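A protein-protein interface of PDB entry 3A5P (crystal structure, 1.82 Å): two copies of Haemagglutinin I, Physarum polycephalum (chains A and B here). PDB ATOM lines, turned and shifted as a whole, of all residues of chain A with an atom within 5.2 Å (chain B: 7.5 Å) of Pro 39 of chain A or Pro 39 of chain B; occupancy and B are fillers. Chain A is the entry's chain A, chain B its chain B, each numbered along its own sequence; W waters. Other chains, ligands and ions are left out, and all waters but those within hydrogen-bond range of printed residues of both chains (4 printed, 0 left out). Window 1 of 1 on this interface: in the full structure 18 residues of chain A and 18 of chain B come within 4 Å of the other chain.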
ATOM      1  N   TYR A  31     -10.664  22.190  -2.924  1.00  0.00           N
ATOM      2  CA  TYR A  31     -11.790  22.353  -1.994  1.00  0.00           C
ATOM      3  C   TYR A  31     -12.156  23.815  -1.985  1.00  0.00           C
ATOM      4  O   TYR A  31     -11.307  24.670  -1.677  1.00  0.00           O
ATOM      5  CB  TYR A  31     -11.368  21.879  -0.594  1.00  0.00           C
ATOM      6  CG  TYR A  31     -10.937  20.424  -0.562  1.00  0.00           C
ATOM      7  CD1 TYR A  31     -11.877  19.408  -0.370  1.00  0.00           C
ATOM      8  CD2 TYR A  31      -9.610  20.064  -0.762  1.00  0.00           C
ATOM      9  CE1 TYR A  31     -11.507  18.079  -0.352  1.00  0.00           C
ATOM     10  CE2 TYR A  31      -9.218  18.712  -0.759  1.00  0.00           C
ATOM     11  CZ  TYR A  31     -10.175  17.730  -0.541  1.00  0.00           C
ATOM     12  OH  TYR A  31      -9.803  16.405  -0.536  1.00  0.00           O
ATOM     13  N   VAL A  32     -13.396  24.119  -2.369  1.00  0.00           N
ATOM     14  CA  VAL A  32     -13.890  25.490  -2.246  1.00  0.00           C
ATOM     15  C   VAL A  32     -14.718  25.576  -0.973  1.00  0.00           C
ATOM     16  O   VAL A  32     -15.721  24.859  -0.820  1.00  0.00           O
ATOM     17  CB  VAL A  32     -14.710  25.966  -3.480  1.00  0.00           C
ATOM     18  CG1 VAL A  32     -15.254  27.371  -3.236  1.00  0.00           C
ATOM     19  CG2 VAL A  32     -13.822  25.982  -4.704  1.00  0.00           C
ATOM     20  N   THR A  33     -14.281  26.452  -0.071  1.00  0.00           N
ATOM     21  CA  THR A  33     -14.856  26.540   1.259  1.00  0.00           C
ATOM     22  C   THR A  33     -15.590  27.861   1.440  1.00  0.00           C
ATOM     23  O   THR A  33     -15.131  28.892   0.958  1.00  0.00           O
ATOM     24  CB  THR A  33     -13.769  26.403   2.362  1.00  0.00           C
ATOM     25  OG1 THR A  33     -12.778  27.450   2.207  1.00  0.00           O
ATOM     26  CG2 THR A  33     -13.122  24.988   2.295  1.00  0.00           C
ATOM     27  N   TYR A  37     -20.849  26.575   5.598  1.00  0.00           N
ATOM     28  CA  TYR A  37     -21.333  25.561   4.674  1.00  0.00           C
ATOM     29  C   TYR A  37     -20.346  24.427   4.488  1.00  0.00           C
ATOM     30  O   TYR A  37     -19.162  24.575   4.783  1.00  0.00           O
ATOM     31  CB  TYR A  37     -21.597  26.195   3.306  1.00  0.00           C
ATOM     32  CG  TYR A  37     -22.622  27.305   3.383  1.00  0.00           C
ATOM     33  CD1 TYR A  37     -23.987  27.015   3.291  1.00  0.00           C
ATOM     34  CD2 TYR A  37     -22.225  28.624   3.582  1.00  0.00           C
ATOM     35  CE1 TYR A  37     -24.945  28.031   3.378  1.00  0.00           C
ATOM     36  CE2 TYR A  37     -23.172  29.659   3.667  1.00  0.00           C
ATOM     37  CZ  TYR A  37     -24.525  29.343   3.564  1.00  0.00           C
ATOM     38  OH  TYR A  37     -25.469  30.332   3.635  1.00  0.00           O
ATOM     39  N   ALA A  38     -20.853  23.320   3.933  1.00  0.00           N
ATOM     40  CA  ALA A  38     -20.018  22.174   3.555  1.00  0.00           C
ATOM     41  C   ALA A  38     -19.099  22.538   2.385  1.00  0.00           C
ATOM     42  O   ALA A  38     -19.538  23.228   1.446  1.00  0.00           O
ATOM     43  CB  ALA A  38     -20.888  20.980   3.223  1.00  0.00           C
ATOM     44  N   PRO A  39     -17.807  22.116   2.445  1.00  0.00           N
ATOM     45  CA  PRO A  39     -16.916  22.350   1.310  1.00  0.00           C
ATOM     46  C   PRO A  39     -17.449  21.681   0.043  1.00  0.00           C
ATOM     47  O   PRO A  39     -18.121  20.642   0.114  1.00  0.00           O
ATOM     48  CB  PRO A  39     -15.586  21.699   1.739  1.00  0.00           C
ATOM     49  CG  PRO A  39     -15.628  21.733   3.263  1.00  0.00           C
ATOM     50  CD  PRO A  39     -17.106  21.467   3.573  1.00  0.00           C
ATOM     51  N   ILE A  40     -17.192  22.319  -1.088  1.00  0.00           N
ATOM     52  CA  ILE A  40     -17.400  21.713  -2.390  1.00  0.00           C
ATOM     53  C   ILE A  40     -16.060  21.108  -2.808  1.00  0.00           C
ATOM     54  O   ILE A  40     -15.068  21.826  -2.874  1.00  0.00           O
ATOM     55  CB  ILE A  40     -17.830  22.779  -3.432  1.00  0.00           C
ATOM     56  CG1 ILE A  40     -19.061  23.571  -2.946  1.00  0.00           C
ATOM     57  CG2 ILE A  40     -18.006  22.153  -4.863  1.00  0.00           C
ATOM     58  CD1 ILE A  40     -19.258  24.856  -3.717  1.00  0.00           C
ATOM     59  N   THR A  41     -16.031  19.799  -3.070  1.00  0.00           N
ATOM     60  CA  THR A  41     -14.798  19.111  -3.475  1.00  0.00           C
ATOM     61  C   THR A  41     -14.761  18.906  -4.994  1.00  0.00           C
ATOM     62  O   THR A  41     -15.752  18.495  -5.600  1.00  0.00           O
ATOM     63  CB  THR A  41     -14.630  17.719  -2.747  1.00  0.00           C
ATOM     64  OG1 THR A  41     -14.656  17.917  -1.330  1.00  0.00           O
ATOM     65  CG2 THR A  41     -13.300  17.032  -3.158  1.00  0.00           C
ATOM     66  N   HIS A  59     -18.247  17.194  -5.721  1.00  0.00           N
ATOM     67  CA  HIS A  59     -19.055  16.776  -4.583  1.00  0.00           C
ATOM     68  C   HIS A  59     -19.529  17.988  -3.781  1.00  0.00           C
ATOM     69  O   HIS A  59     -18.739  18.888  -3.439  1.00  0.00           O
ATOM     70  CB  HIS A  59     -18.282  15.802  -3.690  1.00  0.00           C
ATOM     71  CG  HIS A  59     -18.206  14.422  -4.253  1.00  0.00           C
ATOM     72  ND1 HIS A  59     -17.286  14.062  -5.209  1.00  0.00           N
ATOM     73  CD2 HIS A  59     -18.959  13.321  -4.013  1.00  0.00           C
ATOM     74  CE1 HIS A  59     -17.470  12.794  -5.537  1.00  0.00           C
ATOM     75  NE2 HIS A  59     -18.472  12.319  -4.818  1.00  0.00           N
ATOM     76  N   ASN A  60     -20.821  18.029  -3.508  1.00  0.00           N
ATOM     77  CA  ASN A  60     -21.391  19.073  -2.653  1.00  0.00           C
ATOM     78  C   ASN A  60     -21.520  18.475  -1.246  1.00  0.00           C
ATOM     79  O   ASN A  60     -22.451  17.708  -0.957  1.00  0.00           O
ATOM     80  CB  ASN A  60     -22.735  19.540  -3.229  1.00  0.00           C
ATOM     81  CG  ASN A  60     -23.275  20.794  -2.549  1.00  0.00           C
ATOM     82  OD1 ASN A  60     -22.631  21.381  -1.666  1.00  0.00           O
ATOM     83  ND2 ASN A  60     -24.475  21.201  -2.954  1.00  0.00           N
ATOM     84  N   GLY A  61     -20.553  18.788  -0.376  1.00  0.00           N
ATOM     85  CA  GLY A  61     -20.440  18.072   0.892  1.00  0.00           C
ATOM     86  C   GLY A  61     -20.189  16.607   0.562  1.00  0.00           C
ATOM     87  O   GLY A  61     -19.263  16.291  -0.221  1.00  0.00           O
ATOM     88  N   ARG B  30     -11.714  25.717  10.332  1.00  0.00           N
ATOM     89  CA  ARG B  30     -10.550  24.958   9.879  1.00  0.00           C
ATOM     90  C   ARG B  30     -11.024  23.727   9.117  1.00  0.00           C
ATOM     91  O   ARG B  30     -12.096  23.183   9.412  1.00  0.00           O
ATOM     92  CB  ARG B  30      -9.667  24.528  11.069  1.00  0.00           C
ATOM     93  CG  ARG B  30      -8.384  25.360  11.326  1.00  0.00           C
ATOM     94  CD  ARG B  30      -8.570  26.902  11.248  1.00  0.00           C
ATOM     95  NE  ARG B  30      -9.451  27.498  12.282  1.00  0.00           N
ATOM     96  CZ  ARG B  30      -9.095  27.728  13.557  1.00  0.00           C
ATOM     97  NH1 ARG B  30      -7.899  27.322  14.009  1.00  0.00           N
ATOM     98  NH2 ARG B  30      -9.953  28.317  14.410  1.00  0.00           N
ATOM     99  N   TYR B  31     -10.219  23.280   8.148  1.00  0.00           N
ATOM    100  CA  TYR B  31     -10.600  22.180   7.278  1.00  0.00           C
ATOM    101  C   TYR B  31      -9.443  21.183   7.193  1.00  0.00           C
ATOM    102  O   TYR B  31      -8.291  21.591   7.028  1.00  0.00           O
ATOM    103  CB  TYR B  31     -10.912  22.707   5.877  1.00  0.00           C
ATOM    104  CG  TYR B  31     -12.027  23.704   5.869  1.00  0.00           C
ATOM    105  CD1 TYR B  31     -13.362  23.289   5.913  1.00  0.00           C
ATOM    106  CD2 TYR B  31     -11.748  25.075   5.821  1.00  0.00           C
ATOM    107  CE1 TYR B  31     -14.406  24.237   5.919  1.00  0.00           C
ATOM    108  CE2 TYR B  31     -12.768  26.015   5.831  1.00  0.00           C
ATOM    109  CZ  TYR B  31     -14.093  25.589   5.879  1.00  0.00           C
ATOM    110  OH  TYR B  31     -15.110  26.530   5.881  1.00  0.00           O
ATOM    111  N   VAL B  32      -9.754  19.902   7.376  1.00  0.00           N
ATOM    112  CA  VAL B  32      -8.741  18.854   7.239  1.00  0.00           C
ATOM    113  C   VAL B  32      -9.166  17.944   6.085  1.00  0.00           C
ATOM    114  O   VAL B  32     -10.301  17.466   6.033  1.00  0.00           O
ATOM    115  CB  VAL B  32      -8.531  18.074   8.553  1.00  0.00           C
ATOM    116  CG1 VAL B  32      -7.600  16.864   8.346  1.00  0.00           C
ATOM    117  CG2 VAL B  32      -7.962  19.009   9.646  1.00  0.00           C
ATOM    118  N   THR B  33      -8.244  17.706   5.164  1.00  0.00           N
ATOM    119  CA  THR B  33      -8.571  16.982   3.932  1.00  0.00           C
ATOM    120  C   THR B  33      -7.714  15.739   3.837  1.00  0.00           C
ATOM    121  O   THR B  33      -6.547  15.738   4.262  1.00  0.00           O
ATOM    122  CB  THR B  33      -8.384  17.851   2.660  1.00  0.00           C
ATOM    123  OG1 THR B  33      -7.000  18.246   2.532  1.00  0.00           O
ATOM    124  CG2 THR B  33      -9.296  19.107   2.718  1.00  0.00           C
ATOM    125  N   VAL B  34      -8.319  14.678   3.304  1.00  0.00           N
ATOM    126  CA  VAL B  34      -7.619  13.421   3.049  1.00  0.00           C
ATOM    127  C   VAL B  34      -8.055  12.983   1.653  1.00  0.00           C
ATOM    128  O   VAL B  34      -9.247  12.771   1.412  1.00  0.00           O
ATOM    129  CB  VAL B  34      -7.942  12.327   4.111  1.00  0.00           C
ATOM    130  CG1 VAL B  34      -7.100  11.071   3.885  1.00  0.00           C
ATOM    131  CG2 VAL B  34      -7.738  12.871   5.547  1.00  0.00           C
ATOM    132  N   GLY B  36      -9.461  11.627  -1.437  1.00  0.00           N
ATOM    133  CA  GLY B  36     -10.495  10.642  -1.769  1.00  0.00           C
ATOM    134  C   GLY B  36     -11.648  10.545  -0.788  1.00  0.00           C
ATOM    135  O   GLY B  36     -12.583   9.771  -1.024  1.00  0.00           O
ATOM    136  N   TYR B  37     -11.575  11.318   0.301  1.00  0.00           N
ATOM    137  CA  TYR B  37     -12.577  11.307   1.383  1.00  0.00           C
ATOM    138  C   TYR B  37     -13.245  12.666   1.548  1.00  0.00           C
ATOM    139  O   TYR B  37     -12.696  13.676   1.122  1.00  0.00           O
ATOM    140  CB  TYR B  37     -11.913  10.918   2.722  1.00  0.00           C
ATOM    141  CG  TYR B  37     -11.349   9.518   2.697  1.00  0.00           C
ATOM    142  CD1 TYR B  37     -12.123   8.434   3.123  1.00  0.00           C
ATOM    143  CD2 TYR B  37     -10.055   9.271   2.224  1.00  0.00           C
ATOM    144  CE1 TYR B  37     -11.626   7.125   3.101  1.00  0.00           C
ATOM    145  CE2 TYR B  37      -9.544   7.948   2.175  1.00  0.00           C
ATOM    146  CZ  TYR B  37     -10.349   6.885   2.620  1.00  0.00           C
ATOM    147  OH  TYR B  37      -9.885   5.578   2.593  1.00  0.00           O
ATOM    148  N   ALA B  38     -14.426  12.694   2.174  1.00  0.00           N
ATOM    149  CA  ALA B  38     -15.057  13.981   2.520  1.00  0.00           C
ATOM    150  C   ALA B  38     -14.197  14.731   3.548  1.00  0.00           C
ATOM    151  O   ALA B  38     -13.686  14.117   4.472  1.00  0.00           O
ATOM    152  CB  ALA B  38     -16.461  13.780   3.048  1.00  0.00           C
ATOM    153  N   PRO B  39     -14.001  16.052   3.349  1.00  0.00           N
ATOM    154  CA  PRO B  39     -13.189  16.847   4.277  1.00  0.00           C
ATOM    155  C   PRO B  39     -13.880  17.000   5.638  1.00  0.00           C
ATOM    156  O   PRO B  39     -15.113  16.869   5.746  1.00  0.00           O
ATOM    157  CB  PRO B  39     -13.018  18.201   3.541  1.00  0.00           C
ATOM    158  CG  PRO B  39     -14.140  18.276   2.569  1.00  0.00           C
ATOM    159  CD  PRO B  39     -14.517  16.850   2.220  1.00  0.00           C
ATOM    160  N   ILE B  40     -13.079  17.223   6.669  1.00  0.00           N
ATOM    161  CA  ILE B  40     -13.586  17.437   8.014  1.00  0.00           C
ATOM    162  C   ILE B  40     -13.550  18.932   8.267  1.00  0.00           C
ATOM    163  O   ILE B  40     -12.544  19.577   7.993  1.00  0.00           O
ATOM    164  CB  ILE B  40     -12.716  16.757   9.083  1.00  0.00           C
ATOM    165  CG1 ILE B  40     -12.554  15.255   8.799  1.00  0.00           C
ATOM    166  CG2 ILE B  40     -13.280  17.048  10.510  1.00  0.00           C
ATOM    167  CD1 ILE B  40     -11.434  14.629   9.661  1.00  0.00           C
ATOM    168  N   THR B  41     -14.655  19.483   8.760  1.00  0.00           N
ATOM    169  CA  THR B  41     -14.712  20.901   9.085  1.00  0.00           C
ATOM    170  C   THR B  41     -14.760  21.067  10.585  1.00  0.00           C
ATOM    171  O   THR B  41     -15.500  20.348  11.267  1.00  0.00           O
ATOM    172  CB  THR B  41     -15.940  21.583   8.460  1.00  0.00           C
ATOM    173  OG1 THR B  41     -15.861  21.485   7.041  1.00  0.00           O
ATOM    174  CG2 THR B  41     -16.042  23.094   8.883  1.00  0.00           C
ATOM    175  N   PHE B  42     -13.969  22.020  11.079  1.00  0.00           N
ATOM    176  CA  PHE B  42     -13.971  22.427  12.479  1.00  0.00           C
ATOM    177  C   PHE B  42     -14.502  23.864  12.521  1.00  0.00           C
ATOM    178  O   PHE B  42     -13.945  24.735  11.863  1.00  0.00           O
ATOM    179  CB  PHE B  42     -12.520  22.424  13.026  1.00  0.00           C
ATOM    180  CG  PHE B  42     -11.854  21.078  13.023  1.00  0.00           C
ATOM    181  CD1 PHE B  42     -11.701  20.361  14.222  1.00  0.00           C
ATOM    182  CD2 PHE B  42     -11.356  20.530  11.840  1.00  0.00           C
ATOM    183  CE1 PHE B  42     -11.056  19.110  14.240  1.00  0.00           C
ATOM    184  CE2 PHE B  42     -10.700  19.285  11.838  1.00  0.00           C
ATOM    185  CZ  PHE B  42     -10.554  18.577  13.033  1.00  0.00           C
ATOM    186  N   HIS B  59     -17.725  18.631  11.714  1.00  0.00           N
ATOM    187  CA  HIS B  59     -18.559  18.039  10.674  1.00  0.00           C
ATOM    188  C   HIS B  59     -17.721  17.065   9.842  1.00  0.00           C
ATOM    189  O   HIS B  59     -16.617  17.400   9.397  1.00  0.00           O
ATOM    190  CB  HIS B  59     -19.164  19.139   9.787  1.00  0.00           C
ATOM    191  CG  HIS B  59     -20.310  19.853  10.441  1.00  0.00           C
ATOM    192  ND1 HIS B  59     -20.133  20.873  11.353  1.00  0.00           N
ATOM    193  CD2 HIS B  59     -21.646  19.645  10.362  1.00  0.00           C
ATOM    194  CE1 HIS B  59     -21.316  21.280  11.789  1.00  0.00           C
ATOM    195  NE2 HIS B  59     -22.248  20.543  11.212  1.00  0.00           N
ATOM    196  N   ASN B  60     -18.256  15.864   9.654  1.00  0.00           N
ATOM    197  CA  ASN B  60     -17.636  14.856   8.806  1.00  0.00           C
ATOM    198  C   ASN B  60     -18.354  14.969   7.468  1.00  0.00           C
ATOM    199  O   ASN B  60     -19.512  14.554   7.349  1.00  0.00           O
ATOM    200  CB  ASN B  60     -17.825  13.473   9.460  1.00  0.00           C
ATOM    201  CG  ASN B  60     -17.036  12.372   8.760  1.00  0.00           C
ATOM    202  OD1 ASN B  60     -16.354  12.622   7.771  1.00  0.00           O
ATOM    203  ND2 ASN B  60     -17.149  11.144   9.260  1.00  0.00           N
ATOM    204  N   GLY B  61     -17.711  15.600   6.480  1.00  0.00           N
ATOM    205  CA  GLY B  61     -18.440  16.017   5.271  1.00  0.00           C
ATOM    206  C   GLY B  61     -19.542  16.996   5.672  1.00  0.00           C
ATOM    207  O   GLY B  61     -19.277  17.980   6.372  1.00  0.00           O
ATOM    208  N   ASP B  62     -20.778  16.725   5.262  1.00  0.00           N
ATOM    209  CA  ASP B  62     -21.880  17.638   5.593  1.00  0.00           C
ATOM    210  C   ASP B  62     -22.624  17.247   6.887  1.00  0.00           C
ATOM    211  O   ASP B  62     -23.496  17.984   7.340  1.00  0.00           O
ATOM    212  CB  ASP B  62     -22.809  17.881   4.363  1.00  0.00           C
ATOM    213  CG  ASP B  62     -23.412  16.621   3.828  1.00  0.00           C
ATOM    214  OD1 ASP B  62     -23.967  15.864   4.647  1.00  0.00           O
ATOM    215  OD2 ASP B  62     -23.321  16.368   2.599  1.00  0.00           O
ATOM    216  N   ASP B  63     -22.230  16.135   7.509  1.00  0.00           N
ATOM    217  CA  ASP B  63     -22.895  15.615   8.728  1.00  0.00           C
ATOM    218  C   ASP B  63     -22.226  16.117  10.016  1.00  0.00           C
ATOM    219  O   ASP B  63     -20.993  16.134  10.100  1.00  0.00           O
ATOM    220  CB  ASP B  63     -22.894  14.076   8.757  1.00  0.00           C
ATOM    221  CG  ASP B  63     -23.764  13.459   7.681  1.00  0.00           C
ATOM    222  OD1 ASP B  63     -24.925  13.883   7.503  1.00  0.00           O
ATOM    223  OD2 ASP B  63     -23.283  12.529   7.000  1.00  0.00           O
ATOM    224  N   LEU B 100     -13.504   8.455   8.420  1.00  0.00           N
ATOM    225  CA  LEU B 100     -13.544   9.113   7.110  1.00  0.00           C
ATOM    226  C   LEU B 100     -14.474   8.396   6.132  1.00  0.00           C
ATOM    227  O   LEU B 100     -14.521   7.159   6.100  1.00  0.00           O
ATOM    228  CB  LEU B 100     -12.134   9.187   6.513  1.00  0.00           C
ATOM    229  CG  LEU B 100     -11.118  10.046   7.286  1.00  0.00           C
ATOM    230  CD1 LEU B 100      -9.722   9.957   6.664  1.00  0.00           C
ATOM    231  CD2 LEU B 100     -11.584  11.500   7.391  1.00  0.00           C
ATOM    232  N   LYS B 101     -15.184   9.184   5.332  1.00  0.00           N
ATOM    233  CA  LYS B 101     -16.110   8.665   4.324  1.00  0.00           C
ATOM    234  C   LYS B 101     -15.582   8.898   2.915  1.00  0.00           C
ATOM    235  O   LYS B 101     -15.224  10.033   2.548  1.00  0.00           O
ATOM    236  CB  LYS B 101     -17.466   9.363   4.468  1.00  0.00           C
ATOM    237  CG  LYS B 101     -18.161   9.157   5.794  1.00  0.00           C
ATOM    238  CD  LYS B 101     -19.497   9.926   5.818  1.00  0.00           C
ATOM    239  CE  LYS B 101     -19.293  11.429   5.943  1.00  0.00           C
ATOM    240  NZ  LYS B 101     -20.579  12.185   6.202  1.00  0.00           N
ATOM    241  N   LEU B 103     -15.607   9.646  -0.927  1.00  0.00           N
ATOM    242  CA  LEU B 103     -16.469  10.360  -1.855  1.00  0.00           C
ATOM    243  C   LEU B 103     -16.809   9.403  -3.013  1.00  0.00           C
ATOM    244  O   LEU B 103     -15.916   8.860  -3.641  1.00  0.00           O
ATOM    245  CB  LEU B 103     -15.789  11.633  -2.355  1.00  0.00           C
ATOM    246  CG  LEU B 103     -15.612  12.719  -1.285  1.00  0.00           C
ATOM    247  CD1 LEU B 103     -14.811  13.911  -1.846  1.00  0.00           C
ATOM    248  CD2 LEU B 103     -16.953  13.171  -0.655  1.00  0.00           C
HETATM  249  O   HOH W   1     -17.714  25.972   7.032  1.00  0.00           O
HETATM  250  O   HOH W   2     -16.754  25.217   3.560  1.00  0.00           O
HETATM  251  O   HOH W   3     -11.113  14.082  -1.319  1.00  0.00           O
HETATM  252  O   HOH W   4     -10.902  15.535   2.171  1.00  0.00           O
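Thr 33 of chain B touches Tyr 31 of chain A. Tyr 31 of chain A touches Pro 39 of chain B. Tyr 31 of chain B touches Thr 33 of chain A (CZ to CB, 3.6 Å). Ala 38 of chain A touches Asp 62 of chain B. Tyr 31 of chain B touches Pro 39 of chain A (CD1 to CG, 3.8 Å). CG of Pro 39 of chain B touches CB of Pro 39 of chain A, 3.8 Å away. Pro 39 of chain A touches Thr 41 of chain B (CD to OG1, 3.7 Å). CG2 of Thr 41 of chain A touches CD1 of Leu 103 of chain B, at 3.7 Å. NE2 of His 59 of chain A touches CB of Leu 103 of chain B, at 3.7 Å. O of Asn 60 of chain A touches OD2 of Asp 62 of chain B, 3.9 Å away.
The backbone carbonyl oxygen (O) of Pro 39 of chain A lies within hydrogen-bond range of the backbone NH (N) of Gly 61 of chain A. N of His 59 of chain A sits at hydrogen-bond distance from O of Thr 41 of chain A (2.8 Å). The backbone carbonyl oxygen (O) of Gly 36 of chain B is in hydrogen-bond range of the backbone NH (N) of Leu 103 of chain B. The backbone carbonyl oxygen (O) of Pro 39 of chain B sits at hydrogen-bond distance from the backbone NH (N) of Gly 61 of chain B, 3.0 Å away. The backbone NH of His 59 of chain B lies within hydrogen-bond range of the backbone carbonyl oxygen of Thr 41 of chain B, 2.8 Å away.
Water W2 bridges the backbone carbonyl oxygen (O) of Tyr 37 of chain A (2.8 Å) and the side-chain hydroxyl (OH) of Tyr 31 of chain B (3.1 Å). Water W3 lies within hydrogen-bond range of the side-chain hydroxyl (OH) of Tyr 31 of chain A, the backbone carbonyl oxygen (O) of Tyr 37 of chain B and the backbone NH (N) of Gly 36 of chain B. Water W4 lies within hydrogen-bond range of the backbone carbonyl oxygen of Tyr 37 of chain B (2.8 Å), the backbone NH of Val 34 of chain B (2.9 Å) and the side-chain hydroxyl of Tyr 31 of chain A (3.0 Å). Water W1 lies within hydrogen-bond range of OH of Tyr 31 of chain B (2.9 Å) and O of Tyr 37 of chain A (3.0 Å).
Tyr 31 of chain A touches Thr 33 of chain B, and with the chains exchanged Thr 33 of chain A touches Tyr 31 of chain B. Tyr 31 of chain A touches Pro 39 of chain B, and with the chains exchanged Pro 39 of chain A touches Tyr 31 of chain B. Pro 39 of chain B touches its own counterpart, Pro 39 of chain A. Pro 39 of chain A touches Thr 41 of chain B, and with the chains exchanged Thr 41 of chain A touches Pro 39 of chain B. Positions printed for both chains: 31, 32, 33, 37, 38, 39, 40, 41, 59, 60 and 61.
Hydrophobic or aromatic side chains of chain A that line the printed part of chain B: Tyr 31, Ala 38, Pro 39 and His 59. Hydrophobic or aromatic side chains of chain B that line the printed part of chain A: Tyr 31, Pro 39 and Leu 103. Among the printed residues, no Asp or Glu carboxylate lies within 4 Å of a Lys or Arg side-chain nitrogen of the other chain.
Printed residues of chain B within 4 Å of Tyr 31 of chain A: Thr 33 and Pro 39. Of the printed residues of chain B, Thr 33 of chain A touches Tyr 31 (3.6 Å). Of chain B, only Tyr 31, Pro 39 and Thr 41 come within 4 Å of Pro 39 of chain A. Of the printed residues of chain B, His 59 of chain A touches Leu 103. Gly 36 of chain B touches none of the printed residues of chain A. Of chain A, only Tyr 31, Pro 39 and Thr 41 come within 4 Å of Pro 39 of chain B. Of the printed residues of chain A, Thr 41 of chain B touches Pro 39. Asn 60 of chain B touches none of the printed residues of chain A. Printed residues of chain A within 4 Å of Asp 62 of chain B: Ala 38 (3.8 Å), Asn 60 (3.9 Å) and Gly 61 (3.7 Å).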
